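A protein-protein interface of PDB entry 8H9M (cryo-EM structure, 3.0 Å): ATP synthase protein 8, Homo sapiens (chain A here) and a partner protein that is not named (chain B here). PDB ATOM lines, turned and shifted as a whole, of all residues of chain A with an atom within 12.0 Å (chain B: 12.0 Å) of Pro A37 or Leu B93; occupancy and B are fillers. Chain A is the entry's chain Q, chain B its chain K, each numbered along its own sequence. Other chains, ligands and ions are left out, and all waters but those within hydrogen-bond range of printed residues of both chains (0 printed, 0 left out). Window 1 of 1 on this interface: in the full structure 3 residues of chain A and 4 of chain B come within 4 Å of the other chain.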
ATOM      1  N   ASN A  32     -15.156   9.205  12.956  1.00  0.00           N
ATOM      2  CA  ASN A  32     -15.593   9.142  11.572  1.00  0.00           C
ATOM      3  C   ASN A  32     -15.148   7.833  10.939  1.00  0.00           C
ATOM      4  O   ASN A  32     -14.008   7.398  11.122  1.00  0.00           O
ATOM      5  CB  ASN A  32     -15.042  10.322  10.771  1.00  0.00           C
ATOM      6  CG  ASN A  32     -15.924  11.547  10.865  1.00  0.00           C
ATOM      7  OD1 ASN A  32     -15.454  12.643  11.168  1.00  0.00           O
ATOM      8  ND2 ASN A  32     -17.215  11.365  10.608  1.00  0.00           N
ATOM      9  N   TYR A  33     -16.055   7.212  10.193  1.00  0.00           N
ATOM     10  CA  TYR A  33     -15.793   5.961   9.494  1.00  0.00           C
ATOM     11  C   TYR A  33     -15.819   6.243   7.998  1.00  0.00           C
ATOM     12  O   TYR A  33     -16.885   6.500   7.428  1.00  0.00           O
ATOM     13  CB  TYR A  33     -16.819   4.899   9.877  1.00  0.00           C
ATOM     14  CG  TYR A  33     -16.811   4.559  11.347  1.00  0.00           C
ATOM     15  CD1 TYR A  33     -15.870   3.685  11.869  1.00  0.00           C
ATOM     16  CD2 TYR A  33     -17.741   5.114  12.215  1.00  0.00           C
ATOM     17  CE1 TYR A  33     -15.856   3.371  13.208  1.00  0.00           C
ATOM     18  CE2 TYR A  33     -17.734   4.806  13.557  1.00  0.00           C
ATOM     19  CZ  TYR A  33     -16.789   3.934  14.049  1.00  0.00           C
ATOM     20  OH  TYR A  33     -16.774   3.621  15.386  1.00  0.00           O
ATOM     21  N   HIS A  34     -14.650   6.196   7.367  1.00  0.00           N
ATOM     22  CA  HIS A  34     -14.546   6.514   5.955  1.00  0.00           C
ATOM     23  C   HIS A  34     -15.024   5.343   5.101  1.00  0.00           C
ATOM     24  O   HIS A  34     -15.164   4.210   5.567  1.00  0.00           O
ATOM     25  CB  HIS A  34     -13.110   6.886   5.595  1.00  0.00           C
ATOM     26  CG  HIS A  34     -12.133   5.771   5.794  1.00  0.00           C
ATOM     27  ND1 HIS A  34     -11.981   4.743   4.889  1.00  0.00           N
ATOM     28  CD2 HIS A  34     -11.259   5.521   6.796  1.00  0.00           C
ATOM     29  CE1 HIS A  34     -11.053   3.909   5.323  1.00  0.00           C
ATOM     30  NE2 HIS A  34     -10.598   4.359   6.478  1.00  0.00           N
ATOM     31  N   LEU A  35     -15.276   5.633   3.833  1.00  0.00           N
ATOM     32  CA  LEU A  35     -15.714   4.605   2.907  1.00  0.00           C
ATOM     33  C   LEU A  35     -14.520   3.770   2.448  1.00  0.00           C
ATOM     34  O   LEU A  35     -13.423   4.299   2.256  1.00  0.00           O
ATOM     35  CB  LEU A  35     -16.403   5.233   1.701  1.00  0.00           C
ATOM     36  CG  LEU A  35     -17.909   5.494   1.798  1.00  0.00           C
ATOM     37  CD1 LEU A  35     -18.237   6.462   2.920  1.00  0.00           C
ATOM     38  CD2 LEU A  35     -18.440   6.020   0.478  1.00  0.00           C
ATOM     39  N   PRO A  36     -14.705   2.465   2.273  1.00  0.00           N
ATOM     40  CA  PRO A  36     -13.583   1.599   1.899  1.00  0.00           C
ATOM     41  C   PRO A  36     -13.086   1.926   0.504  1.00  0.00           C
ATOM     42  O   PRO A  36     -13.881   2.270  -0.383  1.00  0.00           O
ATOM     43  CB  PRO A  36     -14.185   0.186   1.959  1.00  0.00           C
ATOM     44  CG  PRO A  36     -15.468   0.329   2.717  1.00  0.00           C
ATOM     45  CD  PRO A  36     -15.956   1.709   2.433  1.00  0.00           C
ATOM     46  N   PRO A  37     -11.780   1.831   0.268  1.00  0.00           N
ATOM     47  CA  PRO A  37     -11.245   2.147  -1.058  1.00  0.00           C
ATOM     48  C   PRO A  37     -11.599   1.070  -2.071  1.00  0.00           C
ATOM     49  O   PRO A  37     -12.157   0.021  -1.744  1.00  0.00           O
ATOM     50  CB  PRO A  37      -9.729   2.217  -0.833  1.00  0.00           C
ATOM     51  CG  PRO A  37      -9.521   2.099   0.652  1.00  0.00           C
ATOM     52  CD  PRO A  37     -10.725   1.419   1.204  1.00  0.00           C
ATOM     53  N   SER A  38     -11.260   1.350  -3.325  1.00  0.00           N
ATOM     54  CA  SER A  38     -11.513   0.413  -4.413  1.00  0.00           C
ATOM     55  C   SER A  38     -10.640  -0.831  -4.277  1.00  0.00           C
ATOM     56  O   SER A  38     -11.052  -1.933  -4.638  1.00  0.00           O
ATOM     57  CB  SER A  38     -11.265   1.082  -5.765  1.00  0.00           C
ATOM     58  OG  SER A  38      -9.912   0.944  -6.162  1.00  0.00           O
ATOM     59  N   LYS B  84      -4.626  -6.852  15.242  1.00  0.00           N
ATOM     60  CA  LYS B  84      -5.084  -7.522  14.032  1.00  0.00           C
ATOM     61  C   LYS B  84      -6.041  -6.645  13.241  1.00  0.00           C
ATOM     62  O   LYS B  84      -6.020  -6.657  12.008  1.00  0.00           O
ATOM     63  CB  LYS B  84      -5.748  -8.848  14.395  1.00  0.00           C
ATOM     64  CG  LYS B  84      -5.992  -9.765  13.216  1.00  0.00           C
ATOM     65  CD  LYS B  84      -6.580 -11.090  13.666  1.00  0.00           C
ATOM     66  CE  LYS B  84      -5.770 -11.699  14.798  1.00  0.00           C
ATOM     67  NZ  LYS B  84      -4.333 -11.842  14.440  1.00  0.00           N
ATOM     68  N   LEU B  85      -6.898  -5.890  13.929  1.00  0.00           N
ATOM     69  CA  LEU B  85      -7.724  -4.902  13.242  1.00  0.00           C
ATOM     70  C   LEU B  85      -6.851  -3.905  12.493  1.00  0.00           C
ATOM     71  O   LEU B  85      -7.097  -3.595  11.319  1.00  0.00           O
ATOM     72  CB  LEU B  85      -8.625  -4.182  14.244  1.00  0.00           C
ATOM     73  CG  LEU B  85      -9.990  -4.806  14.535  1.00  0.00           C
ATOM     74  CD1 LEU B  85     -10.796  -3.912  15.461  1.00  0.00           C
ATOM     75  CD2 LEU B  85     -10.746  -5.063  13.244  1.00  0.00           C
ATOM     76  N   ASN B  86      -5.811  -3.401  13.162  1.00  0.00           N
ATOM     77  CA  ASN B  86      -4.916  -2.446  12.519  1.00  0.00           C
ATOM     78  C   ASN B  86      -4.221  -3.060  11.310  1.00  0.00           C
ATOM     79  O   ASN B  86      -4.115  -2.421  10.257  1.00  0.00           O
ATOM     80  CB  ASN B  86      -3.887  -1.932  13.524  1.00  0.00           C
ATOM     81  CG  ASN B  86      -4.327  -0.653  14.200  1.00  0.00           C
ATOM     82  OD1 ASN B  86      -5.265   0.007  13.753  1.00  0.00           O
ATOM     83  ND2 ASN B  86      -3.650  -0.293  15.283  1.00  0.00           N
ATOM     84  N   GLU B  87      -3.750  -4.304  11.435  1.00  0.00           N
ATOM     85  CA  GLU B  87      -3.030  -4.927  10.327  1.00  0.00           C
ATOM     86  C   GLU B  87      -3.966  -5.258   9.172  1.00  0.00           C
ATOM     87  O   GLU B  87      -3.569  -5.170   8.007  1.00  0.00           O
ATOM     88  CB  GLU B  87      -2.290  -6.185  10.788  1.00  0.00           C
ATOM     89  CG  GLU B  87      -1.427  -6.043  12.047  1.00  0.00           C
ATOM     90  CD  GLU B  87      -0.211  -5.132  11.894  1.00  0.00           C
ATOM     91  OE1 GLU B  87       0.798  -5.389  12.582  1.00  0.00           O
ATOM     92  OE2 GLU B  87      -0.252  -4.156  11.115  1.00  0.00           O
ATOM     93  N   GLN B  88      -5.210  -5.638   9.468  1.00  0.00           N
ATOM     94  CA  GLN B  88      -6.181  -5.861   8.403  1.00  0.00           C
ATOM     95  C   GLN B  88      -6.462  -4.572   7.647  1.00  0.00           C
ATOM     96  O   GLN B  88      -6.491  -4.561   6.409  1.00  0.00           O
ATOM     97  CB  GLN B  88      -7.474  -6.438   8.977  1.00  0.00           C
ATOM     98  CG  GLN B  88      -8.639  -6.433   7.998  1.00  0.00           C
ATOM     99  CD  GLN B  88      -9.987  -6.379   8.689  1.00  0.00           C
ATOM    100  OE1 GLN B  88     -10.239  -5.504   9.517  1.00  0.00           O
ATOM    101  NE2 GLN B  88     -10.865  -7.315   8.349  1.00  0.00           N
ATOM    102  N   LYS B  89      -6.663  -3.469   8.374  1.00  0.00           N
ATOM    103  CA  LYS B  89      -6.893  -2.194   7.704  1.00  0.00           C
ATOM    104  C   LYS B  89      -5.681  -1.780   6.879  1.00  0.00           C
ATOM    105  O   LYS B  89      -5.824  -1.289   5.753  1.00  0.00           O
ATOM    106  CB  LYS B  89      -7.241  -1.113   8.724  1.00  0.00           C
ATOM    107  CG  LYS B  89      -7.838   0.139   8.104  1.00  0.00           C
ATOM    108  CD  LYS B  89      -8.357   1.087   9.168  1.00  0.00           C
ATOM    109  CE  LYS B  89      -8.997   2.310   8.546  1.00  0.00           C
ATOM    110  NZ  LYS B  89      -9.537   3.228   9.584  1.00  0.00           N
ATOM    111  N   LEU B  90      -4.477  -1.985   7.418  1.00  0.00           N
ATOM    112  CA  LEU B  90      -3.266  -1.621   6.689  1.00  0.00           C
ATOM    113  C   LEU B  90      -3.102  -2.460   5.429  1.00  0.00           C
ATOM    114  O   LEU B  90      -2.738  -1.937   4.369  1.00  0.00           O
ATOM    115  CB  LEU B  90      -2.047  -1.775   7.597  1.00  0.00           C
ATOM    116  CG  LEU B  90      -0.788  -1.021   7.173  1.00  0.00           C
ATOM    117  CD1 LEU B  90      -1.099   0.442   6.921  1.00  0.00           C
ATOM    118  CD2 LEU B  90       0.293  -1.168   8.229  1.00  0.00           C
ATOM    119  N   ALA B  91      -3.359  -3.766   5.527  1.00  0.00           N
ATOM    120  CA  ALA B  91      -3.259  -4.633   4.360  1.00  0.00           C
ATOM    121  C   ALA B  91      -4.271  -4.238   3.299  1.00  0.00           C
ATOM    122  O   ALA B  91      -3.938  -4.169   2.112  1.00  0.00           O
ATOM    123  CB  ALA B  91      -3.450  -6.093   4.769  1.00  0.00           C
ATOM    124  N   GLN B  92      -5.514  -3.969   3.706  1.00  0.00           N
ATOM    125  CA  GLN B  92      -6.525  -3.531   2.750  1.00  0.00           C
ATOM    126  C   GLN B  92      -6.111  -2.235   2.065  1.00  0.00           C
ATOM    127  O   GLN B  92      -6.208  -2.112   0.836  1.00  0.00           O
ATOM    128  CB  GLN B  92      -7.867  -3.364   3.458  1.00  0.00           C
ATOM    129  CG  GLN B  92      -9.009  -2.942   2.559  1.00  0.00           C
ATOM    130  CD  GLN B  92     -10.319  -2.827   3.312  1.00  0.00           C
ATOM    131  OE1 GLN B  92     -10.375  -3.057   4.520  1.00  0.00           O
ATOM    132  NE2 GLN B  92     -11.382  -2.467   2.602  1.00  0.00           N
ATOM    133  N   LEU B  93      -5.634  -1.259   2.841  1.00  0.00           N
ATOM    134  CA  LEU B  93      -5.235   0.022   2.267  1.00  0.00           C
ATOM    135  C   LEU B  93      -4.091  -0.152   1.275  1.00  0.00           C
ATOM    136  O   LEU B  93      -4.150   0.354   0.149  1.00  0.00           O
ATOM    137  CB  LEU B  93      -4.845   0.994   3.378  1.00  0.00           C
ATOM    138  CG  LEU B  93      -6.000   1.745   4.040  1.00  0.00           C
ATOM    139  CD1 LEU B  93      -5.479   2.638   5.146  1.00  0.00           C
ATOM    140  CD2 LEU B  93      -6.770   2.556   3.016  1.00  0.00           C
ATOM    141  N   GLU B  94      -3.036  -0.866   1.679  1.00  0.00           N
ATOM    142  CA  GLU B  94      -1.913  -1.095   0.775  1.00  0.00           C
ATOM    143  C   GLU B  94      -2.338  -1.876  -0.460  1.00  0.00           C
ATOM    144  O   GLU B  94      -1.785  -1.669  -1.545  1.00  0.00           O
ATOM    145  CB  GLU B  94      -0.787  -1.823   1.507  1.00  0.00           C
ATOM    146  CG  GLU B  94       0.328  -0.912   1.998  1.00  0.00           C
ATOM    147  CD  GLU B  94       1.271  -0.484   0.889  1.00  0.00           C
ATOM    148  OE1 GLU B  94       2.107   0.412   1.131  1.00  0.00           O
ATOM    149  OE2 GLU B  94       1.180  -1.045  -0.224  1.00  0.00           O
ATOM    150  N   GLU B  95      -3.316  -2.774  -0.318  1.00  0.00           N
ATOM    151  CA  GLU B  95      -3.849  -3.483  -1.473  1.00  0.00           C
ATOM    152  C   GLU B  95      -4.578  -2.536  -2.414  1.00  0.00           C
ATOM    153  O   GLU B  95      -4.551  -2.731  -3.634  1.00  0.00           O
ATOM    154  CB  GLU B  95      -4.776  -4.605  -1.004  1.00  0.00           C
ATOM    155  CG  GLU B  95      -5.810  -5.054  -2.017  1.00  0.00           C
ATOM    156  CD  GLU B  95      -6.558  -6.288  -1.563  1.00  0.00           C
ATOM    157  OE1 GLU B  95      -6.072  -7.409  -1.822  1.00  0.00           O
ATOM    158  OE2 GLU B  95      -7.630  -6.139  -0.942  1.00  0.00           O
ATOM    159  N   ALA B  96      -5.219  -1.504  -1.872  1.00  0.00           N
ATOM    160  CA  ALA B  96      -5.848  -0.492  -2.710  1.00  0.00           C
ATOM    161  C   ALA B  96      -4.858   0.530  -3.253  1.00  0.00           C
ATOM    162  O   ALA B  96      -5.288   1.526  -3.843  1.00  0.00           O
ATOM    163  CB  ALA B  96      -6.952   0.223  -1.932  1.00  0.00           C
ATOM    164  N   LYS B  97      -3.559   0.314  -3.073  1.00  0.00           N
ATOM    165  CA  LYS B  97      -2.549   1.233  -3.590  1.00  0.00           C
ATOM    166  C   LYS B  97      -1.925   0.695  -4.871  1.00  0.00           C
ATOM    167  O   LYS B  97      -1.735  -0.513  -5.021  1.00  0.00           O
ATOM    168  CB  LYS B  97      -1.463   1.484  -2.542  1.00  0.00           C
ATOM    169  CG  LYS B  97      -0.234   2.199  -3.077  1.00  0.00           C
ATOM    170  CD  LYS B  97      -0.407   3.707  -3.028  1.00  0.00           C
ATOM    171  CE  LYS B  97       0.237   4.299  -1.784  1.00  0.00           C
ATOM    172  NZ  LYS B  97      -0.008   5.765  -1.672  1.00  0.00           N
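Printed residues of chain B within 4 Å of His A34: Lys B89 (3.3 Å). Of chain B, only Gln B92 comes within 4 Å of Pro A36. Of chain B, only Leu B93 and Ala B96 come within 4 Å of Pro A37. No residue of chain B comes within 4 Å of Ser A38. No residue of chain A comes within 4 Å of Leu B90. Of the printed residues of chain A, Leu B93 touches Pro A37. No residue of chain A comes within 4 Å of Glu B94. No residue of chain A comes within 4 Å of Glu B95. Of chain A, only Pro A37 (3.6 Å) comes within 4 Å of Ala B96. Lys B97 touches none of the printed residues of chain A. The nearest residue of chain A that does not touch Leu B93 is His A34 (5.0 Å). The nearest printed residue of chain B that does not touch His A34 is Leu B93 (5.0 Å).
Among the printed residues, merely in contact across the chains: Pro A36 with Gln B92, Pro A37 with Leu B93 and Pro A37 with Ala B96.
Printed residues of chain B that touch a printed residue of chain A: Lys B89, Gln B92, Leu B93 and Ala B96. Hydrophobic or aromatic side chains of chain B that line the printed part of chain A: Leu B93 and Ala B96. Of the 7 printed residues of chain A, 3 touch a printed residue of chain B. Hydrophobic or aromatic side chains of chain A that line the printed part of chain B: His A34, Pro A36 and Pro A37. Among the printed residues, 4 pairs touch across the chains.
The side-chain amino group (NZ) of Lys B89 lies close to a ring nitrogen (NE2) of His A34, at 3.5 Å.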
